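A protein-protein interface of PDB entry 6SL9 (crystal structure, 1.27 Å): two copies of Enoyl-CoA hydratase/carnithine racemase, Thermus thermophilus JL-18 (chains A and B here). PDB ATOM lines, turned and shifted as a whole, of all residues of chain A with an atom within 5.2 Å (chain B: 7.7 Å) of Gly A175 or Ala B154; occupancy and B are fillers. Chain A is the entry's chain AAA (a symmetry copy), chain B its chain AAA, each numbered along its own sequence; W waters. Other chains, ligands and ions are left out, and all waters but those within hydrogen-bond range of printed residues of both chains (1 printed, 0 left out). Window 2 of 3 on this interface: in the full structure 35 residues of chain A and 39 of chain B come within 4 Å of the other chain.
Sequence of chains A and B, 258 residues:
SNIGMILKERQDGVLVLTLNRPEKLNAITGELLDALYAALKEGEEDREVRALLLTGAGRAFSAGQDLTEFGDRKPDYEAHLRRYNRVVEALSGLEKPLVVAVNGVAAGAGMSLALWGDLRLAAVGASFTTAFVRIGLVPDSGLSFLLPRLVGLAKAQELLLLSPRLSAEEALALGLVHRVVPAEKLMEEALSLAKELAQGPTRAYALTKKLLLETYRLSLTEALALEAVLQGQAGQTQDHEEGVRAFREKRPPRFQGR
Gly A175 touches just one residue of chain B: Ala B154.
Of chain A, only Arg A120, Leu A150, Gly A175 and His A178 come within 4 Å of Ala B154.
Printed residues of chain A within 4 Å of Gly B152: Arg A149 (3.96 Å).
Printed residues of chain B within 4 Å of Arg A149: Gly B152 (3.96 Å) and Leu B153 (3.0 Å).
Pro B148 touches none of the printed residues of chain A.
The nearest residue of chain B that does not touch Gly A175 is Gln B157 (6.0 Å).
The side-chain carboxylate of Glu B158 lies within salt-bridge range of the side-chain amino group of Lys B155 (3.4 Å).
The backbone carbonyl oxygen (O) of Gly A175 lies within hydrogen-bond range of the guanidinium group (NH2) of Arg A120 (3.0 Å).
The backbone carbonyl oxygen (O) of Leu A176 lies within hydrogen-bond range of the guanidinium group (NE) of Arg A120, 2.8 Å away.
The backbone NH (N) of His A178 lies within hydrogen-bond range of the backbone carbonyl oxygen (O) of Arg A120, at 2.7 Å.
The backbone carbonyl oxygen (O) of Arg A149 sits at hydrogen-bond distance from the backbone NH (N) of Leu B153.
A ring nitrogen (NE2) of His A178 lies within hydrogen-bond range of the backbone carbonyl oxygen (O) of Ala B154, 2.9 Å away.
The side-chain amide oxygen (OE1) of Gln B157 is in hydrogen-bond range of the guanidinium group (NH1) of Arg A120 (2.9 Å).
Of the 12 printed residues of chain A, 5 touch a printed residue of chain B.
Hydrophobic or aromatic side chains of chain B that line the printed part of chain A: Leu B153 and Ala B154.
Among the printed residues, 11 pairs touch across the chains.
Arg A120 touches Ala B154 (NH2 to CB, 3.6 Å).
Arg A149 touches Gly B152 (O to C, 3.96 Å).
CD2 of Leu B153 touches CD2 of Leu A150 (3.8 Å).
Ala B154 touches Leu A150.
Leu A150 touches Gln B157.
CB of Ala B154 touches O of Gly A175, 3.3 Å away.
Gln B157 touches His A178 (OE1 to CE1, 3.8 Å).
Glu B158 touches His A178 (OE1 to CD2, 3.5 Å).
Water W1 lies within hydrogen-bond range of the side-chain carboxylate (OE1) of Glu B158, the side-chain amino group (NZ) of Lys B155 and the backbone carbonyl oxygen (O) of His A178.
Position printed for both chains: 151.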
ATOM      1  N   ARG A 120      23.268   2.397 -21.753  1.00  0.00           N
ATOM      2  CA  ARG A 120      22.225   3.146 -22.477  1.00  0.00           C
ATOM      3  C   ARG A 120      21.770   4.327 -21.634  1.00  0.00           C
ATOM      4  O   ARG A 120      21.440   4.174 -20.458  1.00  0.00           O
ATOM      5  CB  ARG A 120      21.075   2.184 -22.743  1.00  0.00           C
ATOM      6  CG  ARG A 120      21.468   0.999 -23.605  1.00  0.00           C
ATOM      7  CD  ARG A 120      20.373  -0.020 -23.839  1.00  0.00           C
ATOM      8  NE  ARG A 120      19.857  -0.577 -22.597  1.00  0.00           N
ATOM      9  CZ  ARG A 120      20.463  -1.533 -21.900  1.00  0.00           C
ATOM     10  NH1 ARG A 120      21.545  -2.134 -22.378  1.00  0.00           N
ATOM     11  NH2 ARG A 120      19.919  -1.952 -20.753  1.00  0.00           N
ATOM     12  N   ARG A 149      15.098 -10.433 -21.473  1.00  0.00           N
ATOM     13  CA  ARG A 149      16.348 -10.468 -20.671  1.00  0.00           C
ATOM     14  C   ARG A 149      16.519  -9.136 -19.904  1.00  0.00           C
ATOM     15  O   ARG A 149      17.016  -9.132 -18.753  1.00  0.00           O
ATOM     16  CB  ARG A 149      17.522 -10.724 -21.665  1.00  0.00           C
ATOM     17  CG  ARG A 149      17.506 -12.149 -22.250  1.00  0.00           C
ATOM     18  CD  ARG A 149      18.468 -12.333 -23.391  1.00  0.00           C
ATOM     19  NE  ARG A 149      18.761 -13.687 -23.805  1.00  0.00           N
ATOM     20  CZ  ARG A 149      17.873 -14.492 -24.365  1.00  0.00           C
ATOM     21  NH1 ARG A 149      16.713 -13.970 -24.741  1.00  0.00           N
ATOM     22  NH2 ARG A 149      18.189 -15.752 -24.726  1.00  0.00           N
ATOM     23  N   LEU A 150      16.186  -8.000 -20.539  1.00  0.00           N
ATOM     24  CA  LEU A 150      16.419  -6.677 -19.937  1.00  0.00           C
ATOM     25  C   LEU A 150      15.359  -6.343 -18.892  1.00  0.00           C
ATOM     26  O   LEU A 150      15.739  -5.689 -17.901  1.00  0.00           O
ATOM     27  CB  LEU A 150      16.458  -5.602 -21.018  1.00  0.00           C
ATOM     28  CG  LEU A 150      17.625  -5.670 -21.993  1.00  0.00           C
ATOM     29  CD1 LEU A 150      17.417  -4.656 -23.089  1.00  0.00           C
ATOM     30  CD2 LEU A 150      18.953  -5.431 -21.287  1.00  0.00           C
ATOM     31  N   VAL A 151      14.097  -6.706 -19.067  1.00  0.00           N
ATOM     32  CA  VAL A 151      13.002  -6.191 -18.216  1.00  0.00           C
ATOM     33  C   VAL A 151      12.263  -7.364 -17.544  1.00  0.00           C
ATOM     34  O   VAL A 151      11.404  -7.073 -16.728  1.00  0.00           O
ATOM     35  CB  VAL A 151      12.007  -5.267 -18.955  1.00  0.00           C
ATOM     36  CG1 VAL A 151      12.708  -4.089 -19.615  1.00  0.00           C
ATOM     37  CG2 VAL A 151      11.166  -6.010 -19.982  1.00  0.00           C
ATOM     38  N   ALA A 171      11.418   3.951 -18.531  1.00  0.00           N
ATOM     39  CA  ALA A 171      12.464   3.124 -19.145  1.00  0.00           C
ATOM     40  C   ALA A 171      13.563   2.856 -18.126  1.00  0.00           C
ATOM     41  O   ALA A 171      14.105   1.740 -18.049  1.00  0.00           O
ATOM     42  CB  ALA A 171      13.000   3.779 -20.372  1.00  0.00           C
ATOM     43  N   LEU A 172      13.929   3.892 -17.379  1.00  0.00           N
ATOM     44  CA  LEU A 172      14.982   3.738 -16.365  1.00  0.00           C
ATOM     45  C   LEU A 172      14.528   2.734 -15.300  1.00  0.00           C
ATOM     46  O   LEU A 172      15.280   1.848 -14.941  1.00  0.00           O
ATOM     47  CB  LEU A 172      15.247   5.109 -15.745  1.00  0.00           C
ATOM     48  CG  LEU A 172      16.295   5.125 -14.653  1.00  0.00           C
ATOM     49  CD1 LEU A 172      17.685   4.742 -15.150  1.00  0.00           C
ATOM     50  CD2 LEU A 172      16.334   6.481 -14.015  1.00  0.00           C
ATOM     51  N   ALA A 173      13.314   2.850 -14.809  1.00  0.00           N
ATOM     52  CA  ALA A 173      12.816   1.946 -13.750  1.00  0.00           C
ATOM     53  C   ALA A 173      12.801   0.503 -14.258  1.00  0.00           C
ATOM     54  O   ALA A 173      13.035  -0.421 -13.446  1.00  0.00           O
ATOM     55  CB  ALA A 173      11.455   2.331 -13.275  1.00  0.00           C
ATOM     56  N   LEU A 174      12.578   0.270 -15.548  1.00  0.00           N
ATOM     57  CA  LEU A 174      12.494  -1.106 -16.087  1.00  0.00           C
ATOM     58  C   LEU A 174      13.864  -1.686 -16.428  1.00  0.00           C
ATOM     59  O   LEU A 174      13.899  -2.944 -16.604  1.00  0.00           O
ATOM     60  CB  LEU A 174      11.632  -1.074 -17.355  1.00  0.00           C
ATOM     61  CG  LEU A 174      10.164  -0.729 -17.140  1.00  0.00           C
ATOM     62  CD1 LEU A 174       9.409  -0.902 -18.425  1.00  0.00           C
ATOM     63  CD2 LEU A 174       9.533  -1.573 -16.017  1.00  0.00           C
ATOM     64  N   GLY A 175      14.911  -0.863 -16.563  1.00  0.00           N
ATOM     65  CA  GLY A 175      16.206  -1.324 -17.120  1.00  0.00           C
ATOM     66  C   GLY A 175      16.343  -1.136 -18.619  1.00  0.00           C
ATOM     67  O   GLY A 175      17.405  -1.494 -19.174  1.00  0.00           O
ATOM     68  N   LEU A 176      15.408  -0.516 -19.306  1.00  0.00           N
ATOM     69  CA  LEU A 176      15.637  -0.186 -20.738  1.00  0.00           C
ATOM     70  C   LEU A 176      16.794   0.794 -20.885  1.00  0.00           C
ATOM     71  O   LEU A 176      17.526   0.725 -21.909  1.00  0.00           O
ATOM     72  CB  LEU A 176      14.372   0.387 -21.342  1.00  0.00           C
ATOM     73  CG  LEU A 176      13.201  -0.584 -21.424  1.00  0.00           C
ATOM     74  CD1 LEU A 176      11.989   0.107 -21.993  1.00  0.00           C
ATOM     75  CD2 LEU A 176      13.512  -1.855 -22.194  1.00  0.00           C
ATOM     76  N   VAL A 177      16.973   1.683 -19.919  1.00  0.00           N
ATOM     77  CA  VAL A 177      18.195   2.537 -19.907  1.00  0.00           C
ATOM     78  C   VAL A 177      18.813   2.491 -18.525  1.00  0.00           C
ATOM     79  O   VAL A 177      18.119   2.117 -17.552  1.00  0.00           O
ATOM     80  CB  VAL A 177      17.913   3.973 -20.358  1.00  0.00           C
ATOM     81  CG1 VAL A 177      17.445   4.038 -21.805  1.00  0.00           C
ATOM     82  CG2 VAL A 177      16.988   4.662 -19.400  1.00  0.00           C
ATOM     83  N   HIS A 178      20.078   2.887 -18.452  1.00  0.00           N
ATOM     84  CA  HIS A 178      20.858   2.966 -17.197  1.00  0.00           C
ATOM     85  C   HIS A 178      20.828   4.357 -16.555  1.00  0.00           C
ATOM     86  O   HIS A 178      21.091   4.444 -15.374  1.00  0.00           O
ATOM     87  CB  HIS A 178      22.292   2.515 -17.453  1.00  0.00           C
ATOM     88  CG  HIS A 178      22.391   1.094 -17.942  1.00  0.00           C
ATOM     89  ND1 HIS A 178      22.669   0.814 -19.254  1.00  0.00           N
ATOM     90  CD2 HIS A 178      22.275  -0.083 -17.273  1.00  0.00           C
ATOM     91  CE1 HIS A 178      22.741  -0.515 -19.337  1.00  0.00           C
ATOM     92  NE2 HIS A 178      22.455  -1.088 -18.158  1.00  0.00           N
ATOM     93  N   PRO B 148      23.220 -12.359 -14.416  1.00  0.00           N
ATOM     94  CA  PRO B 148      22.063 -11.952 -15.194  1.00  0.00           C
ATOM     95  C   PRO B 148      20.761 -12.612 -14.721  1.00  0.00           C
ATOM     96  O   PRO B 148      19.702 -11.983 -14.794  1.00  0.00           O
ATOM     97  CB  PRO B 148      22.412 -12.350 -16.614  1.00  0.00           C
ATOM     98  CG  PRO B 148      23.882 -12.704 -16.608  1.00  0.00           C
ATOM     99  CD  PRO B 148      24.265 -13.030 -15.228  1.00  0.00           C
ATOM    100  N   VAL B 151      19.774 -10.551 -11.301  1.00  0.00           N
ATOM    101  CA  VAL B 151      19.533  -9.092 -11.310  1.00  0.00           C
ATOM    102  C   VAL B 151      18.995  -8.656 -12.686  1.00  0.00           C
ATOM    103  O   VAL B 151      18.651  -7.491 -12.793  1.00  0.00           O
ATOM    104  CB  VAL B 151      20.764  -8.246 -10.909  1.00  0.00           C
ATOM    105  CG1 VAL B 151      21.308  -8.643  -9.545  1.00  0.00           C
ATOM    106  CG2 VAL B 151      21.878  -8.298 -11.944  1.00  0.00           C
ATOM    107  N   GLY B 152      18.901  -9.548 -13.667  1.00  0.00           N
ATOM    108  CA  GLY B 152      18.510  -9.221 -15.045  1.00  0.00           C
ATOM    109  C   GLY B 152      19.692  -8.727 -15.861  1.00  0.00           C
ATOM    110  O   GLY B 152      20.717  -8.289 -15.318  1.00  0.00           O
ATOM    111  N   LEU B 153      19.561  -8.754 -17.180  1.00  0.00           N
ATOM    112  CA  LEU B 153      20.693  -8.412 -18.059  1.00  0.00           C
ATOM    113  C   LEU B 153      21.081  -6.932 -17.923  1.00  0.00           C
ATOM    114  O   LEU B 153      22.276  -6.607 -17.996  1.00  0.00           O
ATOM    115  CB  LEU B 153      20.330  -8.749 -19.494  1.00  0.00           C
ATOM    116  CG  LEU B 153      21.377  -8.380 -20.520  1.00  0.00           C
ATOM    117  CD1 LEU B 153      22.689  -9.097 -20.276  1.00  0.00           C
ATOM    118  CD2 LEU B 153      20.866  -8.648 -21.932  1.00  0.00           C
ATOM    119  N   ALA B 154      20.117  -6.041 -17.757  1.00  0.00           N
ATOM    120  CA  ALA B 154      20.458  -4.599 -17.757  1.00  0.00           C
ATOM    121  C   ALA B 154      21.369  -4.263 -16.587  1.00  0.00           C
ATOM    122  O   ALA B 154      22.419  -3.612 -16.762  1.00  0.00           O
ATOM    123  CB  ALA B 154      19.191  -3.771 -17.691  1.00  0.00           C
ATOM    124  N   LYS B 155      21.031  -4.752 -15.415  1.00  0.00           N
ATOM    125  CA  LYS B 155      21.915  -4.487 -14.254  1.00  0.00           C
ATOM    126  C   LYS B 155      23.202  -5.296 -14.338  1.00  0.00           C
ATOM    127  O   LYS B 155      24.243  -4.814 -13.918  1.00  0.00           O
ATOM    128  CB  LYS B 155      21.160  -4.721 -12.954  1.00  0.00           C
ATOM    129  CG  LYS B 155      20.175  -3.632 -12.610  1.00  0.00           C
ATOM    130  CD  LYS B 155      20.910  -2.336 -12.246  1.00  0.00           C
ATOM    131  CE  LYS B 155      20.034  -1.288 -11.638  1.00  0.00           C
ATOM    132  NZ  LYS B 155      20.792  -0.022 -11.522  1.00  0.00           N
ATOM    133  N   ALA B 156      23.141  -6.505 -14.873  1.00  0.00           N
ATOM    134  CA  ALA B 156      24.378  -7.294 -15.023  1.00  0.00           C
ATOM    135  C   ALA B 156      25.357  -6.533 -15.926  1.00  0.00           C
ATOM    136  O   ALA B 156      26.573  -6.496 -15.630  1.00  0.00           O
ATOM    137  CB  ALA B 156      24.065  -8.686 -15.553  1.00  0.00           C
ATOM    138  N   GLN B 157      24.891  -5.915 -17.015  1.00  0.00           N
ATOM    139  CA  GLN B 157      25.807  -5.132 -17.914  1.00  0.00           C
ATOM    140  C   GLN B 157      26.511  -4.063 -17.114  1.00  0.00           C
ATOM    141  O   GLN B 157      27.756  -3.877 -17.242  1.00  0.00           O
ATOM    142  CB  GLN B 157      24.966  -4.450 -19.021  1.00  0.00           C
ATOM    143  CG  GLN B 157      24.546  -5.453 -20.060  1.00  0.00           C
ATOM    144  CD  GLN B 157      23.494  -4.831 -20.983  1.00  0.00           C
ATOM    145  OE1 GLN B 157      22.585  -4.072 -20.562  1.00  0.00           O
ATOM    146  NE2 GLN B 157      23.568  -5.297 -22.195  1.00  0.00           N
ATOM    147  N   GLU B 158      25.734  -3.278 -16.367  1.00  0.00           N
ATOM    148  CA  GLU B 158      26.356  -2.138 -15.647  1.00  0.00           C
ATOM    149  C   GLU B 158      27.338  -2.680 -14.597  1.00  0.00           C
ATOM    150  O   GLU B 158      28.441  -2.163 -14.430  1.00  0.00           O
ATOM    151  CB  GLU B 158      25.213  -1.368 -15.002  1.00  0.00           C
ATOM    152  CG  GLU B 158      25.620  -0.119 -14.264  1.00  0.00           C
ATOM    153  CD  GLU B 158      24.452   0.689 -13.749  1.00  0.00           C
ATOM    154  OE1 GLU B 158      23.248   0.288 -13.925  1.00  0.00           O
ATOM    155  OE2 GLU B 158      24.756   1.745 -13.167  1.00  0.00           O
ATOM    156  N   LEU B 159      26.889  -3.672 -13.821  1.00  0.00           N
ATOM    157  CA  LEU B 159      27.693  -4.153 -12.694  1.00  0.00           C
ATOM    158  C   LEU B 159      28.992  -4.741 -13.216  1.00  0.00           C
ATOM    159  O   LEU B 159      30.002  -4.608 -12.536  1.00  0.00           O
ATOM    160  CB  LEU B 159      26.920  -5.174 -11.872  1.00  0.00           C
ATOM    161  CG  LEU B 159      26.010  -4.601 -10.801  1.00  0.00           C
ATOM    162  CD1 LEU B 159      25.333  -3.263 -10.958  1.00  0.00           C
ATOM    163  CD2 LEU B 159      25.172  -5.708 -10.236  1.00  0.00           C
ATOM    164  N   LEU B 160      28.949  -5.475 -14.316  1.00  0.00           N
ATOM    165  CA  LEU B 160      30.155  -6.127 -14.817  1.00  0.00           C
ATOM    166  C   LEU B 160      31.077  -5.164 -15.555  1.00  0.00           C
ATOM    167  O   LEU B 160      32.324  -5.234 -15.372  1.00  0.00           O
ATOM    168  CB  LEU B 160      29.759  -7.306 -15.722  1.00  0.00           C
ATOM    169  CG  LEU B 160      29.158  -8.481 -14.989  1.00  0.00           C
ATOM    170  CD1 LEU B 160      28.503  -9.399 -15.993  1.00  0.00           C
ATOM    171  CD2 LEU B 160      30.204  -9.238 -14.174  1.00  0.00           C
HETATM  172  O   HOH W   1      21.147   1.723 -13.814  1.00  0.00           O
